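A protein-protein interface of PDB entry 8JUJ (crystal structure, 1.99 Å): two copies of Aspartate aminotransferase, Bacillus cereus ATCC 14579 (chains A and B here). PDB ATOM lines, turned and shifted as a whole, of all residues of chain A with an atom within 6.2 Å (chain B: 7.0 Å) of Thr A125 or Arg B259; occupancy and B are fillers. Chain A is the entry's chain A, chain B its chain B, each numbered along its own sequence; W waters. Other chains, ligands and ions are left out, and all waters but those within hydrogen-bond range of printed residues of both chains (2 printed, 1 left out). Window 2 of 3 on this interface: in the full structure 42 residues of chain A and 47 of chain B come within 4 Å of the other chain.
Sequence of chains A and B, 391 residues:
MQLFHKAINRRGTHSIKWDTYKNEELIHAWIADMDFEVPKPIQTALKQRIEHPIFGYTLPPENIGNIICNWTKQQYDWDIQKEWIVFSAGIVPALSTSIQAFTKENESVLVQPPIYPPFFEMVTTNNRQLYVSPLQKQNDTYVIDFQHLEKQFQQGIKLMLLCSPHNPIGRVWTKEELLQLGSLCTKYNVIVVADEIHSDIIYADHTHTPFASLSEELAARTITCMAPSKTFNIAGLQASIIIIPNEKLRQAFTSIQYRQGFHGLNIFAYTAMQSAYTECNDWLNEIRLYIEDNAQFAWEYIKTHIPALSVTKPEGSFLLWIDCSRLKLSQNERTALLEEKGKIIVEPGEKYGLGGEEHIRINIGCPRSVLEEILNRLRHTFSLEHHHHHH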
ATOM      1  N   SER A  96      -8.086 -10.028 -17.281  1.00  0.00           N
ATOM      2  CA  SER A  96      -8.455  -8.652 -17.680  1.00  0.00           C
ATOM      3  C   SER A  96      -7.844  -8.305 -19.039  1.00  0.00           C
ATOM      4  O   SER A  96      -8.569  -7.808 -19.872  1.00  0.00           O
ATOM      5  CB  SER A  96      -8.043  -7.673 -16.623  1.00  0.00           C
ATOM      6  OG  SER A  96      -8.285  -6.345 -17.069  1.00  0.00           O
ATOM      7  N   THR A  97      -6.558  -8.551 -19.249  1.00  0.00           N
ATOM      8  CA  THR A  97      -5.861  -8.260 -20.534  1.00  0.00           C
ATOM      9  C   THR A  97      -6.533  -9.034 -21.669  1.00  0.00           C
ATOM     10  O   THR A  97      -6.793  -8.455 -22.743  1.00  0.00           O
ATOM     11  CB  THR A  97      -4.375  -8.588 -20.389  1.00  0.00           C
ATOM     12  OG1 THR A  97      -3.982  -7.701 -19.351  1.00  0.00           O
ATOM     13  CG2 THR A  97      -3.554  -8.410 -21.657  1.00  0.00           C
ATOM     14  N   GLN A 100      -9.854  -7.498 -22.586  1.00  0.00           N
ATOM     15  CA  GLN A 100      -9.622  -6.221 -23.322  1.00  0.00           C
ATOM     16  C   GLN A 100      -9.071  -6.516 -24.734  1.00  0.00           C
ATOM     17  O   GLN A 100      -9.423  -5.806 -25.657  1.00  0.00           O
ATOM     18  CB  GLN A 100      -8.707  -5.313 -22.503  1.00  0.00           C
ATOM     19  CG  GLN A 100      -9.370  -4.766 -21.239  1.00  0.00           C
ATOM     20  CD  GLN A 100      -8.569  -3.681 -20.565  1.00  0.00           C
ATOM     21  OE1 GLN A 100      -8.273  -2.648 -21.151  1.00  0.00           O
ATOM     22  NE2 GLN A 100      -8.156  -3.929 -19.327  1.00  0.00           N
ATOM     23  N   PHE A 120     -15.924 -13.100 -12.480  1.00  0.00           N
ATOM     24  CA  PHE A 120     -17.100 -12.214 -12.683  1.00  0.00           C
ATOM     25  C   PHE A 120     -16.631 -10.764 -12.771  1.00  0.00           C
ATOM     26  O   PHE A 120     -17.082 -10.066 -13.698  1.00  0.00           O
ATOM     27  CB  PHE A 120     -18.120 -12.363 -11.558  1.00  0.00           C
ATOM     28  CG  PHE A 120     -18.711 -13.739 -11.371  1.00  0.00           C
ATOM     29  CD1 PHE A 120     -19.683 -14.210 -12.227  1.00  0.00           C
ATOM     30  CD2 PHE A 120     -18.356 -14.520 -10.286  1.00  0.00           C
ATOM     31  CE1 PHE A 120     -20.263 -15.454 -12.037  1.00  0.00           C
ATOM     32  CE2 PHE A 120     -18.933 -15.768 -10.092  1.00  0.00           C
ATOM     33  CZ  PHE A 120     -19.896 -16.227 -10.965  1.00  0.00           C
ATOM     34  N   GLU A 121     -15.808 -10.339 -11.804  1.00  0.00           N
ATOM     35  CA  GLU A 121     -15.382  -8.926 -11.587  1.00  0.00           C
ATOM     36  C   GLU A 121     -14.654  -8.379 -12.820  1.00  0.00           C
ATOM     37  O   GLU A 121     -14.905  -7.240 -13.204  1.00  0.00           O
ATOM     38  CB  GLU A 121     -14.445  -8.833 -10.382  1.00  0.00           C
ATOM     39  CG  GLU A 121     -15.143  -9.128  -9.059  1.00  0.00           C
ATOM     40  CD  GLU A 121     -16.220  -8.099  -8.771  1.00  0.00           C
ATOM     41  OE1 GLU A 121     -15.878  -6.889  -8.612  1.00  0.00           O
ATOM     42  OE2 GLU A 121     -17.413  -8.483  -8.784  1.00  0.00           O
ATOM     43  N   MET A 122     -13.801  -9.183 -13.442  1.00  0.00           N
ATOM     44  CA  MET A 122     -13.019  -8.762 -14.626  1.00  0.00           C
ATOM     45  C   MET A 122     -13.928  -8.611 -15.851  1.00  0.00           C
ATOM     46  O   MET A 122     -13.621  -7.753 -16.707  1.00  0.00           O
ATOM     47  CB  MET A 122     -11.892  -9.766 -14.876  1.00  0.00           C
ATOM     48  CG  MET A 122     -10.813  -9.689 -13.798  1.00  0.00           C
ATOM     49  SD  MET A 122     -10.204  -8.007 -13.451  1.00  0.00           S
ATOM     50  CE  MET A 122     -11.115  -7.609 -11.953  1.00  0.00           C
ATOM     51  N   VAL A 123     -15.015  -9.379 -15.943  1.00  0.00           N
ATOM     52  CA  VAL A 123     -16.058  -9.165 -16.983  1.00  0.00           C
ATOM     53  C   VAL A 123     -16.799  -7.838 -16.751  1.00  0.00           C
ATOM     54  O   VAL A 123     -16.875  -7.046 -17.716  1.00  0.00           O
ATOM     55  CB  VAL A 123     -17.038 -10.340 -17.026  1.00  0.00           C
ATOM     56  CG1 VAL A 123     -18.166 -10.074 -17.992  1.00  0.00           C
ATOM     57  CG2 VAL A 123     -16.309 -11.628 -17.378  1.00  0.00           C
ATOM     58  N   THR A 124     -17.345  -7.616 -15.549  1.00  0.00           N
ATOM     59  CA  THR A 124     -18.337  -6.532 -15.293  1.00  0.00           C
ATOM     60  C   THR A 124     -17.644  -5.173 -15.126  1.00  0.00           C
ATOM     61  O   THR A 124     -18.169  -4.181 -15.652  1.00  0.00           O
ATOM     62  CB  THR A 124     -19.225  -6.903 -14.099  1.00  0.00           C
ATOM     63  OG1 THR A 124     -18.396  -7.026 -12.951  1.00  0.00           O
ATOM     64  CG2 THR A 124     -19.956  -8.206 -14.327  1.00  0.00           C
ATOM     65  N   THR A 125     -16.458  -5.121 -14.525  1.00  0.00           N
ATOM     66  CA  THR A 125     -15.711  -3.854 -14.321  1.00  0.00           C
ATOM     67  C   THR A 125     -15.178  -3.398 -15.686  1.00  0.00           C
ATOM     68  O   THR A 125     -14.826  -2.209 -15.815  1.00  0.00           O
ATOM     69  CB  THR A 125     -14.557  -3.983 -13.316  1.00  0.00           C
ATOM     70  OG1 THR A 125     -13.671  -4.935 -13.895  1.00  0.00           O
ATOM     71  CG2 THR A 125     -14.991  -4.340 -11.906  1.00  0.00           C
ATOM     72  N   ASN A 126     -15.129  -4.289 -16.687  1.00  0.00           N
ATOM     73  CA  ASN A 126     -14.709  -3.891 -18.068  1.00  0.00           C
ATOM     74  C   ASN A 126     -15.904  -3.706 -19.011  1.00  0.00           C
ATOM     75  O   ASN A 126     -15.670  -3.621 -20.218  1.00  0.00           O
ATOM     76  CB  ASN A 126     -13.696  -4.914 -18.601  1.00  0.00           C
ATOM     77  CG  ASN A 126     -12.350  -4.736 -17.936  1.00  0.00           C
ATOM     78  OD1 ASN A 126     -11.627  -3.777 -18.247  1.00  0.00           O
ATOM     79  ND2 ASN A 126     -11.984  -5.646 -17.041  1.00  0.00           N
ATOM     80  N   ASN A 127     -17.139  -3.680 -18.515  1.00  0.00           N
ATOM     81  CA  ASN A 127     -18.342  -3.377 -19.331  1.00  0.00           C
ATOM     82  C   ASN A 127     -18.424  -4.404 -20.483  1.00  0.00           C
ATOM     83  O   ASN A 127     -18.680  -4.014 -21.636  1.00  0.00           O
ATOM     84  CB  ASN A 127     -18.315  -1.900 -19.777  1.00  0.00           C
ATOM     85  CG  ASN A 127     -19.587  -1.452 -20.485  1.00  0.00           C
ATOM     86  OD1 ASN A 127     -20.701  -1.801 -20.058  1.00  0.00           O
ATOM     87  ND2 ASN A 127     -19.453  -0.676 -21.563  1.00  0.00           N
ATOM     88  N   ARG A 128     -18.172  -5.685 -20.196  1.00  0.00           N
ATOM     89  CA  ARG A 128     -18.578  -6.801 -21.086  1.00  0.00           C
ATOM     90  C   ARG A 128     -19.822  -7.442 -20.481  1.00  0.00           C
ATOM     91  O   ARG A 128     -20.055  -7.252 -19.257  1.00  0.00           O
ATOM     92  CB  ARG A 128     -17.453  -7.828 -21.276  1.00  0.00           C
ATOM     93  CG  ARG A 128     -16.505  -7.479 -22.417  1.00  0.00           C
ATOM     94  CD  ARG A 128     -15.665  -6.260 -22.194  1.00  0.00           C
ATOM     95  NE  ARG A 128     -14.619  -6.088 -23.216  1.00  0.00           N
ATOM     96  CZ  ARG A 128     -13.820  -5.037 -23.312  1.00  0.00           C
ATOM     97  NH1 ARG A 128     -13.918  -4.027 -22.451  1.00  0.00           N
ATOM     98  NH2 ARG A 128     -12.915  -4.992 -24.276  1.00  0.00           N
ATOM     99  N   GLN B 100      -6.321   6.823 -18.881  1.00  0.00           N
ATOM    100  CA  GLN B 100      -7.584   6.066 -18.967  1.00  0.00           C
ATOM    101  C   GLN B 100      -8.583   6.576 -17.930  1.00  0.00           C
ATOM    102  O   GLN B 100      -9.761   6.590 -18.241  1.00  0.00           O
ATOM    103  CB  GLN B 100      -7.304   4.587 -18.762  1.00  0.00           C
ATOM    104  CG  GLN B 100      -6.433   4.005 -19.860  1.00  0.00           C
ATOM    105  CD  GLN B 100      -6.253   2.536 -19.623  1.00  0.00           C
ATOM    106  OE1 GLN B 100      -7.185   1.778 -19.852  1.00  0.00           O
ATOM    107  NE2 GLN B 100      -5.093   2.138 -19.087  1.00  0.00           N
ATOM    108  N   ALA B 101      -8.120   7.040 -16.780  1.00  0.00           N
ATOM    109  CA  ALA B 101      -8.983   7.512 -15.680  1.00  0.00           C
ATOM    110  C   ALA B 101      -9.551   8.906 -15.989  1.00  0.00           C
ATOM    111  O   ALA B 101     -10.701   9.135 -15.670  1.00  0.00           O
ATOM    112  CB  ALA B 101      -8.208   7.479 -14.381  1.00  0.00           C
ATOM    113  N   ARG B 128      -5.493   8.589 -27.351  1.00  0.00           N
ATOM    114  CA  ARG B 128      -5.673  10.025 -26.995  1.00  0.00           C
ATOM    115  C   ARG B 128      -4.867  10.869 -27.990  1.00  0.00           C
ATOM    116  O   ARG B 128      -3.933  10.356 -28.598  1.00  0.00           O
ATOM    117  CB  ARG B 128      -5.264  10.289 -25.540  1.00  0.00           C
ATOM    118  CG  ARG B 128      -6.365  10.006 -24.524  1.00  0.00           C
ATOM    119  CD  ARG B 128      -6.793   8.547 -24.456  1.00  0.00           C
ATOM    120  NE  ARG B 128      -7.748   8.364 -23.377  1.00  0.00           N
ATOM    121  CZ  ARG B 128      -8.318   7.204 -23.040  1.00  0.00           C
ATOM    122  NH1 ARG B 128      -8.013   6.096 -23.696  1.00  0.00           N
ATOM    123  NH2 ARG B 128      -9.145   7.144 -22.022  1.00  0.00           N
ATOM    124  N   THR B 254      -8.210   4.277  -9.005  1.00  0.00           N
ATOM    125  CA  THR B 254      -8.178   2.915  -8.403  1.00  0.00           C
ATOM    126  C   THR B 254      -9.219   2.032  -9.106  1.00  0.00           C
ATOM    127  O   THR B 254      -8.954   0.852  -9.187  1.00  0.00           O
ATOM    128  CB  THR B 254      -8.323   2.961  -6.875  1.00  0.00           C
ATOM    129  OG1 THR B 254      -9.580   3.531  -6.538  1.00  0.00           O
ATOM    130  CG2 THR B 254      -7.237   3.746  -6.191  1.00  0.00           C
ATOM    131  N   SER B 255     -10.293   2.600  -9.692  1.00  0.00           N
ATOM    132  CA  SER B 255     -11.235   1.863 -10.575  1.00  0.00           C
ATOM    133  C   SER B 255     -10.522   1.255 -11.770  1.00  0.00           C
ATOM    134  O   SER B 255     -10.871   0.104 -12.106  1.00  0.00           O
ATOM    135  CB  SER B 255     -12.347   2.700 -11.099  1.00  0.00           C
ATOM    136  OG  SER B 255     -13.226   2.877 -10.047  1.00  0.00           O
ATOM    137  N   ILE B 256      -9.687   2.035 -12.460  1.00  0.00           N
ATOM    138  CA  ILE B 256      -8.911   1.541 -13.633  1.00  0.00           C
ATOM    139  C   ILE B 256      -7.958   0.437 -13.147  1.00  0.00           C
ATOM    140  O   ILE B 256      -7.863  -0.597 -13.832  1.00  0.00           O
ATOM    141  CB  ILE B 256      -8.138   2.675 -14.345  1.00  0.00           C
ATOM    142  CG1 ILE B 256      -9.004   3.855 -14.793  1.00  0.00           C
ATOM    143  CG2 ILE B 256      -7.338   2.123 -15.503  1.00  0.00           C
ATOM    144  CD1 ILE B 256      -9.994   3.525 -15.885  1.00  0.00           C
ATOM    145  N   GLN B 257      -7.212   0.662 -12.061  1.00  0.00           N
ATOM    146  CA  GLN B 257      -6.288  -0.357 -11.505  1.00  0.00           C
ATOM    147  C   GLN B 257      -7.063  -1.656 -11.257  1.00  0.00           C
ATOM    148  O   GLN B 257      -6.561  -2.767 -11.568  1.00  0.00           O
ATOM    149  CB  GLN B 257      -5.646   0.123 -10.207  1.00  0.00           C
ATOM    150  CG  GLN B 257      -4.594   1.191 -10.402  1.00  0.00           C
ATOM    151  CD  GLN B 257      -3.965   1.470  -9.065  1.00  0.00           C
ATOM    152  OE1 GLN B 257      -4.670   1.766  -8.110  1.00  0.00           O
ATOM    153  NE2 GLN B 257      -2.659   1.344  -8.982  1.00  0.00           N
ATOM    154  N   TYR B 258      -8.258  -1.528 -10.697  1.00  0.00           N
ATOM    155  CA  TYR B 258      -9.066  -2.690 -10.274  1.00  0.00           C
ATOM    156  C   TYR B 258      -9.473  -3.484 -11.516  1.00  0.00           C
ATOM    157  O   TYR B 258      -9.302  -4.726 -11.531  1.00  0.00           O
ATOM    158  CB  TYR B 258     -10.296  -2.273  -9.465  1.00  0.00           C
ATOM    159  CG  TYR B 258     -11.062  -3.442  -8.908  1.00  0.00           C
ATOM    160  CD1 TYR B 258     -10.687  -4.074  -7.720  1.00  0.00           C
ATOM    161  CD2 TYR B 258     -12.160  -3.921  -9.585  1.00  0.00           C
ATOM    162  CE1 TYR B 258     -11.411  -5.150  -7.219  1.00  0.00           C
ATOM    163  CE2 TYR B 258     -12.887  -4.993  -9.110  1.00  0.00           C
ATOM    164  CZ  TYR B 258     -12.511  -5.612  -7.932  1.00  0.00           C
ATOM    165  OH  TYR B 258     -13.293  -6.651  -7.547  1.00  0.00           O
ATOM    166  N   ARG B 259      -9.958  -2.803 -12.543  1.00  0.00           N
ATOM    167  CA  ARG B 259     -10.476  -3.467 -13.774  1.00  0.00           C
ATOM    168  C   ARG B 259      -9.289  -4.052 -14.548  1.00  0.00           C
ATOM    169  O   ARG B 259      -9.515  -4.888 -15.403  1.00  0.00           O
ATOM    170  CB  ARG B 259     -11.305  -2.473 -14.597  1.00  0.00           C
ATOM    171  CG  ARG B 259     -10.496  -1.605 -15.549  1.00  0.00           C
ATOM    172  CD  ARG B 259     -11.421  -0.672 -16.298  1.00  0.00           C
ATOM    173  NE  ARG B 259     -10.703  -0.024 -17.367  1.00  0.00           N
ATOM    174  CZ  ARG B 259     -11.176   1.003 -18.051  1.00  0.00           C
ATOM    175  NH1 ARG B 259     -12.370   1.465 -17.753  1.00  0.00           N
ATOM    176  NH2 ARG B 259     -10.446   1.572 -18.995  1.00  0.00           N
ATOM    177  N   GLN B 260      -8.050  -3.676 -14.211  1.00  0.00           N
ATOM    178  CA  GLN B 260      -6.829  -4.225 -14.870  1.00  0.00           C
ATOM    179  C   GLN B 260      -6.260  -5.379 -14.023  1.00  0.00           C
ATOM    180  O   GLN B 260      -5.248  -5.955 -14.412  1.00  0.00           O
ATOM    181  CB  GLN B 260      -5.803  -3.120 -15.131  1.00  0.00           C
ATOM    182  CG  GLN B 260      -6.302  -2.146 -16.187  1.00  0.00           C
ATOM    183  CD  GLN B 260      -5.399  -0.992 -16.529  1.00  0.00           C
ATOM    184  OE1 GLN B 260      -5.702  -0.214 -17.426  1.00  0.00           O
ATOM    185  NE2 GLN B 260      -4.287  -0.881 -15.847  1.00  0.00           N
ATOM    186  N   GLY B 261      -6.916  -5.713 -12.920  1.00  0.00           N
ATOM    187  CA  GLY B 261      -6.558  -6.880 -12.087  1.00  0.00           C
ATOM    188  C   GLY B 261      -5.420  -6.593 -11.134  1.00  0.00           C
ATOM    189  O   GLY B 261      -4.870  -7.559 -10.599  1.00  0.00           O
ATOM    190  N   PHE B 262      -5.101  -5.316 -10.886  1.00  0.00           N
ATOM    191  CA  PHE B 262      -4.009  -4.919  -9.957  1.00  0.00           C
ATOM    192  C   PHE B 262      -4.446  -5.140  -8.512  1.00  0.00           C
ATOM    193  O   PHE B 262      -5.489  -4.626  -8.129  1.00  0.00           O
ATOM    194  CB  PHE B 262      -3.616  -3.454 -10.146  1.00  0.00           C
ATOM    195  CG  PHE B 262      -2.530  -2.991  -9.212  1.00  0.00           C
ATOM    196  CD1 PHE B 262      -1.231  -3.454  -9.356  1.00  0.00           C
ATOM    197  CD2 PHE B 262      -2.817  -2.131  -8.154  1.00  0.00           C
ATOM    198  CE1 PHE B 262      -0.233  -3.022  -8.497  1.00  0.00           C
ATOM    199  CE2 PHE B 262      -1.815  -1.705  -7.300  1.00  0.00           C
ATOM    200  CZ  PHE B 262      -0.535  -2.172  -7.462  1.00  0.00           C
HETATM  201  O   HOH W   1      -4.898  -6.089 -17.293  1.00  0.00           O
HETATM  202  O   HOH W   2      -5.951  -0.721 -21.191  1.00  0.00           O
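The backbone carbonyl oxygen (O) of Arg B259 is in hydrogen-bond range of the side-chain hydroxyl (OG) of Ser A96, 2.5 Å away.
OE1 of Glu A121 is in hydrogen-bond range of OH of Tyr B258 (2.8 Å).
ND2 of Asn A126 sits at hydrogen-bond distance from O of Arg B259, at 3.1 Å.
The side-chain sulfur of Met A122 lies close to the backbone carbonyl oxygen of Arg B259 (3.7 Å).
OG of Ser A96 is in hydrogen-bond range of NE2 of Gln A100 (3.3 Å).
The side-chain hydroxyl (OG1) of Thr A125 sits at hydrogen-bond distance from the backbone carbonyl oxygen (O) of Glu A121.
The backbone carbonyl oxygen of Met A122 lies within hydrogen-bond range of the side-chain amide nitrogen of Asn A126, at 2.7 Å.
The backbone carbonyl oxygen (O) of Asn A126 is in hydrogen-bond range of the guanidinium group (NH1) of Arg A128 (2.9 Å).
The side-chain amide oxygen of Gln B100 lies within hydrogen-bond range of the guanidinium group of Arg B259 (3.4 Å).
The side-chain amide nitrogen (NE2) of Gln B100 sits at hydrogen-bond distance from the side-chain amide oxygen (OE1) of Gln B260 (2.9 Å).
Among the printed residues, merely in contact across the chains: Ser A96 with Gln B260 (3.4 Å), Met A122 with Tyr B258 (3.4 Å), Thr A125 with Tyr B258 (3.6 Å) and Thr A125 with Arg B259 (3.5 Å).
Of chain B, only Tyr B258 and Arg B259 come within 4 Å of Thr A125.
Arg B259 touches just these residues of chain A: Ser A96, Met A122, Thr A125 and Asn A126.
Of the printed residues of chain A, Gln B260 touches Ser A96 (3.4 Å).
Printed residues of chain B within 4 Å of Ser A96: Arg B259 and Gln B260.
The nearest printed residue of chain B that does not touch Met A122 is Gly B261 (4.04 Å).
Printed residues of chain B that touch a printed residue of chain A: Tyr B258, Arg B259 and Gln B260.
Hydrophobic or aromatic side chains of chain B that line the printed part of chain A: Tyr B258.
Of the 12 printed residues of chain A, 5 touch a printed residue of chain B.
Hydrophobic or aromatic side chains of chain A that line the printed part of chain B: Met A122.
Along chain A the printed residues that touch a printed residue of chain B span positions 96 to 126.
Among the printed residues, no Asp or Glu carboxylate lies within 4 Å of a Lys or Arg side-chain nitrogen of the other chain.
2 positions are printed for both chains.
Water W1 lies within hydrogen-bond range of OG1 of Thr A97 (2.8 Å), O of Gln B260 (2.9 Å) and OG of Ser A96 (3.4 Å).
Water W2 bridges the side-chain amide oxygen of Gln A100 and the side-chain amide oxygen of Gln B100.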
